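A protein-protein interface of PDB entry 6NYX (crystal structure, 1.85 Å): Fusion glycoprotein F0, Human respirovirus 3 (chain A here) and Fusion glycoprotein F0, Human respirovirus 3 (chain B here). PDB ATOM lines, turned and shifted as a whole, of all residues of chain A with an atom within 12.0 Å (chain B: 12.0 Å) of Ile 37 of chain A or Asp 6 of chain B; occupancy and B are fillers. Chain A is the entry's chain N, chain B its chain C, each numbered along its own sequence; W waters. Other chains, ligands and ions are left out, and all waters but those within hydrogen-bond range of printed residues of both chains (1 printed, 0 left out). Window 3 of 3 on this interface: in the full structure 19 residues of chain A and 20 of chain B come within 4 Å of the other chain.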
ATOM      1  N   ARG A  28      -0.673 -29.684  -7.149  1.00  0.00           N
ATOM      2  CA  ARG A  28      -1.585 -30.392  -6.249  1.00  0.00           C
ATOM      3  C   ARG A  28      -0.869 -31.016  -5.060  1.00  0.00           C
ATOM      4  O   ARG A  28      -1.357 -30.933  -3.928  1.00  0.00           O
ATOM      5  CB  ARG A  28      -2.374 -31.465  -7.010  1.00  0.00           C
ATOM      6  CG  ARG A  28      -3.315 -30.900  -8.116  1.00  0.00           C
ATOM      7  CD  ARG A  28      -4.301 -31.986  -8.644  1.00  0.00           C
ATOM      8  NE  ARG A  28      -3.607 -32.953  -9.491  1.00  0.00           N
ATOM      9  CZ  ARG A  28      -3.543 -32.871 -10.823  1.00  0.00           C
ATOM     10  NH1 ARG A  28      -4.157 -31.888 -11.462  1.00  0.00           N
ATOM     11  NH2 ARG A  28      -2.848 -33.767 -11.489  1.00  0.00           N
ATOM     12  N   ARG A  29       0.313 -31.600  -5.271  1.00  0.00           N
ATOM     13  CA  ARG A  29       1.074 -32.209  -4.187  1.00  0.00           C
ATOM     14  C   ARG A  29       1.595 -31.171  -3.196  1.00  0.00           C
ATOM     15  O   ARG A  29       1.551 -31.392  -1.979  1.00  0.00           O
ATOM     16  CB  ARG A  29       2.261 -33.010  -4.754  1.00  0.00           C
ATOM     17  CG  ARG A  29       1.871 -34.181  -5.558  1.00  0.00           C
ATOM     18  CD  ARG A  29       3.036 -34.970  -6.039  1.00  0.00           C
ATOM     19  NE  ARG A  29       2.544 -36.018  -6.910  1.00  0.00           N
ATOM     20  CZ  ARG A  29       3.279 -37.025  -7.360  1.00  0.00           C
ATOM     21  NH1 ARG A  29       4.558 -37.136  -6.988  1.00  0.00           N
ATOM     22  NH2 ARG A  29       2.731 -37.935  -8.155  1.00  0.00           N
ATOM     23  N   SER A  30       2.095 -30.034  -3.682  1.00  0.00           N
ATOM     24  CA  SER A  30       2.490 -28.950  -2.797  1.00  0.00           C
ATOM     25  C   SER A  30       1.326 -28.471  -1.939  1.00  0.00           C
ATOM     26  O   SER A  30       1.444 -28.375  -0.705  1.00  0.00           O
ATOM     27  CB  SER A  30       3.015 -27.771  -3.603  1.00  0.00           C
ATOM     28  OG  SER A  30       3.408 -26.716  -2.728  1.00  0.00           O
ATOM     29  N   ASN A  31       0.179 -28.181  -2.567  1.00  0.00           N
ATOM     30  CA  ASN A  31      -0.984 -27.747  -1.784  1.00  0.00           C
ATOM     31  C   ASN A  31      -1.454 -28.827  -0.805  1.00  0.00           C
ATOM     32  O   ASN A  31      -1.890 -28.507   0.317  1.00  0.00           O
ATOM     33  CB  ASN A  31      -2.132 -27.345  -2.695  1.00  0.00           C
ATOM     34  CG  ASN A  31      -1.907 -25.997  -3.395  1.00  0.00           C
ATOM     35  OD1 ASN A  31      -1.384 -25.068  -2.820  1.00  0.00           O
ATOM     36  ND2 ASN A  31      -2.314 -25.914  -4.640  1.00  0.00           N
ATOM     37  N   GLN A  32      -1.351 -30.107  -1.180  1.00  0.00           N
ATOM     38  CA  GLN A  32      -1.704 -31.157  -0.226  1.00  0.00           C
ATOM     39  C   GLN A  32      -0.827 -31.086   1.009  1.00  0.00           C
ATOM     40  O   GLN A  32      -1.339 -31.191   2.124  1.00  0.00           O
ATOM     41  CB  GLN A  32      -1.606 -32.537  -0.861  1.00  0.00           C
ATOM     42  CG  GLN A  32      -2.757 -32.816  -1.853  1.00  0.00           C
ATOM     43  CD  GLN A  32      -2.383 -33.847  -2.930  1.00  0.00           C
ATOM     44  OE1 GLN A  32      -1.305 -34.474  -2.883  1.00  0.00           O
ATOM     45  NE2 GLN A  32      -3.262 -34.029  -3.887  1.00  0.00           N
ATOM     46  N   LYS A  33       0.494 -30.909   0.834  1.00  0.00           N
ATOM     47  CA  LYS A  33       1.389 -30.777   1.979  1.00  0.00           C
ATOM     48  C   LYS A  33       1.040 -29.578   2.846  1.00  0.00           C
ATOM     49  O   LYS A  33       1.071 -29.666   4.081  1.00  0.00           O
ATOM     50  CB  LYS A  33       2.833 -30.673   1.522  1.00  0.00           C
ATOM     51  CG  LYS A  33       3.516 -32.020   1.435  1.00  0.00           C
ATOM     52  CD  LYS A  33       4.139 -32.208   0.106  1.00  0.00           C
ATOM     53  CE  LYS A  33       4.320 -33.691  -0.148  1.00  0.00           C
ATOM     54  NZ  LYS A  33       4.639 -33.928  -1.553  1.00  0.00           N
ATOM     55  N   LEU A  34       0.741 -28.436   2.232  1.00  0.00           N
ATOM     56  CA  LEU A  34       0.360 -27.263   3.017  1.00  0.00           C
ATOM     57  C   LEU A  34      -0.961 -27.490   3.758  1.00  0.00           C
ATOM     58  O   LEU A  34      -1.152 -26.966   4.861  1.00  0.00           O
ATOM     59  CB  LEU A  34       0.206 -26.023   2.143  1.00  0.00           C
ATOM     60  CG  LEU A  34       1.381 -25.540   1.305  1.00  0.00           C
ATOM     61  CD1 LEU A  34       1.058 -24.356   0.437  1.00  0.00           C
ATOM     62  CD2 LEU A  34       2.557 -25.194   2.223  1.00  0.00           C
ATOM     63  N   ASP A  35      -1.864 -28.238   3.159  1.00  0.00           N
ATOM     64  CA  ASP A  35      -3.154 -28.588   3.790  1.00  0.00           C
ATOM     65  C   ASP A  35      -2.888 -29.356   5.084  1.00  0.00           C
ATOM     66  O   ASP A  35      -3.720 -29.324   5.920  1.00  0.00           O
ATOM     67  CB  ASP A  35      -4.003 -29.435   2.863  1.00  0.00           C
ATOM     68  CG  ASP A  35      -4.659 -28.638   1.768  1.00  0.00           C
ATOM     69  OD1 ASP A  35      -4.518 -27.439   1.759  1.00  0.00           O
ATOM     70  OD2 ASP A  35      -5.305 -29.241   0.957  1.00  0.00           O
ATOM     71  N   SER A  36      -1.746 -30.013   5.202  1.00  0.00           N
ATOM     72  CA  SER A  36      -1.344 -30.835   6.367  1.00  0.00           C
ATOM     73  C   SER A  36      -0.859 -29.986   7.541  1.00  0.00           C
ATOM     74  O   SER A  36      -0.637 -30.564   8.577  1.00  0.00           O
ATOM     75  CB  SER A  36      -0.282 -31.778   5.986  1.00  0.00           C
ATOM     76  OG  SER A  36      -0.855 -32.893   5.376  1.00  0.00           O
ATOM     77  N   ILE A  37      -0.564 -28.715   7.307  1.00  0.00           N
ATOM     78  CA  ILE A  37      -0.129 -27.719   8.322  1.00  0.00           C
ATOM     79  C   ILE A  37      -1.365 -26.968   8.811  1.00  0.00           C
ATOM     80  O   ILE A  37      -1.664 -27.133   9.991  1.00  0.00           O
ATOM     81  CB  ILE A  37       0.887 -26.740   7.719  1.00  0.00           C
ATOM     82  CG1 ILE A  37       2.095 -27.460   7.138  1.00  0.00           C
ATOM     83  CG2 ILE A  37       1.304 -25.680   8.726  1.00  0.00           C
ATOM     84  CD1 ILE A  37       2.908 -26.579   6.282  1.00  0.00           C
ATOM     85  N   ALA B   3       6.721 -25.988  14.736  1.00  0.00           N
ATOM     86  CA  ALA B   3       7.237 -27.339  15.044  1.00  0.00           C
ATOM     87  C   ALA B   3       8.243 -27.808  13.989  1.00  0.00           C
ATOM     88  O   ALA B   3       8.374 -27.186  12.938  1.00  0.00           O
ATOM     89  CB  ALA B   3       6.089 -28.315  15.135  1.00  0.00           C
ATOM     90  N   ARG B   4       8.922 -28.910  14.281  1.00  0.00           N
ATOM     91  CA  ARG B   4       9.913 -29.516  13.368  1.00  0.00           C
ATOM     92  C   ARG B   4       9.131 -30.202  12.250  1.00  0.00           C
ATOM     93  O   ARG B   4       9.649 -30.284  11.166  1.00  0.00           O
ATOM     94  CB  ARG B   4      10.860 -30.482  14.095  1.00  0.00           C
ATOM     95  N   SER B   5       7.935 -30.700  12.548  1.00  0.00           N
ATOM     96  CA  SER B   5       7.078 -31.388  11.568  1.00  0.00           C
ATOM     97  C   SER B   5       6.598 -30.348  10.577  1.00  0.00           C
ATOM     98  O   SER B   5       6.660 -30.623   9.404  1.00  0.00           O
ATOM     99  CB  SER B   5       5.934 -32.073  12.186  1.00  0.00           C
ATOM    100  OG  SER B   5       5.377 -33.002  11.274  1.00  0.00           O
ATOM    101  N   ASP B   6       6.160 -29.197  11.059  1.00  0.00           N
ATOM    102  CA  ASP B   6       5.651 -28.110  10.194  1.00  0.00           C
ATOM    103  C   ASP B   6       6.807 -27.606   9.331  1.00  0.00           C
ATOM    104  O   ASP B   6       6.572 -27.322   8.193  1.00  0.00           O
ATOM    105  CB  ASP B   6       5.014 -27.003  11.018  1.00  0.00           C
ATOM    106  CG  ASP B   6       3.576 -27.251  11.417  1.00  0.00           C
ATOM    107  OD1 ASP B   6       3.004 -26.355  11.989  1.00  0.00           O
ATOM    108  OD2 ASP B   6       3.045 -28.318  11.130  1.00  0.00           O
ATOM    109  N   ILE B   7       8.022 -27.509   9.862  1.00  0.00           N
ATOM    110  CA  ILE B   7       9.157 -27.084   9.047  1.00  0.00           C
ATOM    111  C   ILE B   7       9.424 -28.101   7.950  1.00  0.00           C
ATOM    112  O   ILE B   7       9.650 -27.752   6.781  1.00  0.00           O
ATOM    113  CB  ILE B   7      10.409 -26.884   9.924  1.00  0.00           C
ATOM    114  CG1 ILE B   7      10.320 -25.593  10.732  1.00  0.00           C
ATOM    115  CG2 ILE B   7      11.635 -26.853   9.083  1.00  0.00           C
ATOM    116  CD1 ILE B   7      11.381 -25.466  11.812  1.00  0.00           C
ATOM    117  N   GLU B   8       9.435 -29.384   8.310  1.00  0.00           N
ATOM    118  CA  GLU B   8       9.630 -30.433   7.302  1.00  0.00           C
ATOM    119  C   GLU B   8       8.522 -30.445   6.253  1.00  0.00           C
ATOM    120  O   GLU B   8       8.773 -30.780   5.083  1.00  0.00           O
ATOM    121  CB  GLU B   8       9.707 -31.816   7.964  1.00  0.00           C
ATOM    122  N   LYS B   9       7.296 -30.112   6.649  1.00  0.00           N
ATOM    123  CA  LYS B   9       6.195 -30.074   5.697  1.00  0.00           C
ATOM    124  C   LYS B   9       6.351 -28.915   4.723  1.00  0.00           C
ATOM    125  O   LYS B   9       6.063 -29.045   3.519  1.00  0.00           O
ATOM    126  CB  LYS B   9       4.865 -29.908   6.422  1.00  0.00           C
ATOM    127  CG  LYS B   9       4.394 -31.141   7.143  1.00  0.00           C
ATOM    128  CD  LYS B   9       3.168 -30.833   7.996  1.00  0.00           C
ATOM    129  CE  LYS B   9       2.742 -32.044   8.797  1.00  0.00           C
ATOM    130  NZ  LYS B   9       1.862 -31.654   9.946  1.00  0.00           N
ATOM    131  N   LEU B  10       6.724 -27.750   5.256  1.00  0.00           N
ATOM    132  CA  LEU B  10       6.906 -26.581   4.402  1.00  0.00           C
ATOM    133  C   LEU B  10       8.030 -26.845   3.414  1.00  0.00           C
ATOM    134  O   LEU B  10       7.939 -26.464   2.245  1.00  0.00           O
ATOM    135  CB  LEU B  10       7.205 -25.355   5.271  1.00  0.00           C
ATOM    136  CG  LEU B  10       6.040 -24.752   6.065  1.00  0.00           C
ATOM    137  CD1 LEU B  10       6.617 -23.737   7.065  1.00  0.00           C
ATOM    138  CD2 LEU B  10       5.027 -24.092   5.210  1.00  0.00           C
ATOM    139  N   LYS B  11       9.102 -27.514   3.870  1.00  0.00           N
ATOM    140  CA  LYS B  11      10.207 -27.874   2.981  1.00  0.00           C
ATOM    141  C   LYS B  11       9.740 -28.802   1.873  1.00  0.00           C
ATOM    142  O   LYS B  11      10.084 -28.605   0.700  1.00  0.00           O
ATOM    143  CB  LYS B  11      11.328 -28.538   3.781  1.00  0.00           C
ATOM    144  CG  LYS B  11      12.487 -29.072   2.988  1.00  0.00           C
ATOM    145  CD  LYS B  11      13.558 -29.622   3.957  1.00  0.00           C
ATOM    146  CE  LYS B  11      14.658 -30.358   3.226  1.00  0.00           C
ATOM    147  NZ  LYS B  11      15.675 -30.943   4.178  1.00  0.00           N
ATOM    148  N   GLU B  12       8.915 -29.775   2.215  1.00  0.00           N
ATOM    149  CA  GLU B  12       8.390 -30.759   1.256  1.00  0.00           C
ATOM    150  C   GLU B  12       7.512 -30.013   0.250  1.00  0.00           C
ATOM    151  O   GLU B  12       7.582 -30.334  -0.904  1.00  0.00           O
ATOM    152  CB  GLU B  12       7.641 -31.891   1.967  1.00  0.00           C
ATOM    153  CG  GLU B  12       8.530 -32.871   2.731  1.00  0.00           C
ATOM    154  CD  GLU B  12       7.807 -33.924   3.572  1.00  0.00           C
ATOM    155  OE1 GLU B  12       6.747 -34.370   3.160  1.00  0.00           O
ATOM    156  OE2 GLU B  12       8.293 -34.273   4.671  1.00  0.00           O
ATOM    157  N   ALA B  13       6.745 -29.037   0.710  1.00  0.00           N
ATOM    158  CA  ALA B  13       5.824 -28.267  -0.137  1.00  0.00           C
ATOM    159  C   ALA B  13       6.637 -27.467  -1.142  1.00  0.00           C
ATOM    160  O   ALA B  13       6.269 -27.463  -2.289  1.00  0.00           O
ATOM    161  CB  ALA B  13       4.942 -27.377   0.672  1.00  0.00           C
ATOM    162  N   ILE B  14       7.662 -26.762  -0.686  1.00  0.00           N
ATOM    163  CA  ILE B  14       8.500 -25.947  -1.603  1.00  0.00           C
ATOM    164  C   ILE B  14       9.186 -26.871  -2.616  1.00  0.00           C
ATOM    165  O   ILE B  14       9.283 -26.478  -3.731  1.00  0.00           O
ATOM    166  CB  ILE B  14       9.498 -25.043  -0.863  1.00  0.00           C
ATOM    167  CG1 ILE B  14       8.821 -24.106   0.121  1.00  0.00           C
ATOM    168  CG2 ILE B  14      10.326 -24.263  -1.844  1.00  0.00           C
ATOM    169  CD1 ILE B  14       9.769 -23.507   1.108  1.00  0.00           C
ATOM    170  N   ARG B  15       9.630 -28.059  -2.225  1.00  0.00           N
ATOM    171  CA  ARG B  15      10.261 -29.006  -3.177  1.00  0.00           C
ATOM    172  C   ARG B  15       9.280 -29.328  -4.300  1.00  0.00           C
ATOM    173  O   ARG B  15       9.694 -29.315  -5.409  1.00  0.00           O
ATOM    174  CB  ARG B  15      10.684 -30.341  -2.566  1.00  0.00           C
ATOM    175  CG  ARG B  15      11.877 -30.220  -1.656  1.00  0.00           C
ATOM    176  CD  ARG B  15      13.133 -30.776  -2.270  1.00  0.00           C
ATOM    177  NE  ARG B  15      14.090 -31.051  -1.227  1.00  0.00           N
ATOM    178  CZ  ARG B  15      15.286 -30.518  -1.161  1.00  0.00           C
ATOM    179  NH1 ARG B  15      15.815 -29.936  -2.224  1.00  0.00           N
ATOM    180  NH2 ARG B  15      15.950 -30.577  -0.025  1.00  0.00           N
ATOM    181  N   ASP B  16       8.021 -29.621  -3.954  1.00  0.00           N
ATOM    182  CA  ASP B  16       6.969 -29.966  -4.948  1.00  0.00           C
ATOM    183  C   ASP B  16       6.744 -28.725  -5.828  1.00  0.00           C
ATOM    184  O   ASP B  16       6.663 -28.852  -6.998  1.00  0.00           O
ATOM    185  CB  ASP B  16       5.669 -30.441  -4.300  1.00  0.00           C
ATOM    186  CG  ASP B  16       5.729 -31.757  -3.541  1.00  0.00           C
ATOM    187  OD1 ASP B  16       6.465 -32.608  -3.932  1.00  0.00           O
ATOM    188  OD2 ASP B  16       5.007 -31.898  -2.612  1.00  0.00           O
ATOM    189  N   THR B  17       6.664 -27.540  -5.234  1.00  0.00           N
ATOM    190  CA  THR B  17       6.488 -26.323  -6.019  1.00  0.00           C
ATOM    191  C   THR B  17       7.660 -26.161  -6.985  1.00  0.00           C
ATOM    192  O   THR B  17       7.470 -25.802  -8.152  1.00  0.00           O
ATOM    193  CB  THR B  17       6.374 -25.100  -5.106  1.00  0.00           C
ATOM    194  OG1 THR B  17       5.192 -25.185  -4.255  1.00  0.00           O
ATOM    195  CG2 THR B  17       6.301 -23.775  -5.907  1.00  0.00           C
HETATM  196  O   HOH W   1      -0.941 -33.163   9.284  1.00  0.00           O
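Water W1 bridges the backbone carbonyl oxygen (O) of Ser 36 of chain A (2.7 Å) and the side-chain amino group (NZ) of Lys 9 of chain B (3.3 Å).
OD2 of Asp 6 of chain B lies within salt-bridge range of NZ of Lys 9 of chain B (3.7 Å). O of Ala 13 of chain B is in hydrogen-bond range of OG1 of Thr 17 of chain B (3.2 Å).
Of the printed residues of chain B, Arg 29 of chain A touches Asp 16. Asn 31 of chain A touches none of the printed residues of chain B. Printed residues of chain B within 4 Å of Lys 33 of chain A: Glu 12 and Asp 16. Of chain B, only Ala 13 (3.6 Å) comes within 4 Å of Leu 34 of chain A. No residue of chain B comes within 4 Å of Asp 35 of chain A. No residue of chain A comes within 4 Å of Arg 4 of chain B. No residue of chain A comes within 4 Å of Ser 5 of chain B. No residue of chain A comes within 4 Å of Glu 8 of chain B. Of the printed residues of chain A, Glu 12 of chain B touches Lys 33 (3.98 Å).
Of the 15 printed residues of chain B, 7 touch a printed residue of chain A. Printed residues of chain B that touch a printed residue of chain A: Asp 6, Lys 9, Leu 10, Glu 12, Ala 13, Asp 16 and Thr 17. Hydrophobic or aromatic side chains of chain B that line the printed part of chain A: Leu 10 and Ala 13. Of the 10 printed residues of chain A, 6 touch a printed residue of chain B. Hydrophobic or aromatic side chains of chain A within 4 Å of the printed part of chain B: Leu 34 and Ile 37. Among the printed residues, Asp or Glu carboxylates within 4 Å of a Lys or Arg side-chain nitrogen of the other chain: Lys 33 of chain A with Asp 16 of chain B (2.3 Å).
Among the printed residues, merely in contact across the chains: Ile 37 of chain A with Leu 10 of chain B, Arg 29 of chain A with Asp 16 of chain B, Leu 34 of chain A with Ala 13 of chain B, Ser 30 of chain A with Asp 16 of chain B, Ile 37 of chain A with Lys 9 of chain B, Ile 37 of chain A with Asp 6 of chain B and Lys 33 of chain A with Glu 12 of chain B.
NZ of Lys 9 of chain B lies within hydrogen-bond range of O of Ser 36 of chain A, at 3.1 Å. The backbone carbonyl oxygen of Ala 13 of chain B is in hydrogen-bond range of the side-chain hydroxyl of Ser 30 of chain A (3.0 Å). OD1 of Asp 16 of chain B is in salt-bridge range of NZ of Lys 33 of chain A, at 3.3 Å. The side-chain hydroxyl (OG1) of Thr 17 of chain B is in hydrogen-bond range of the side-chain hydroxyl (OG) of Ser 30 of chain A (2.8 Å).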
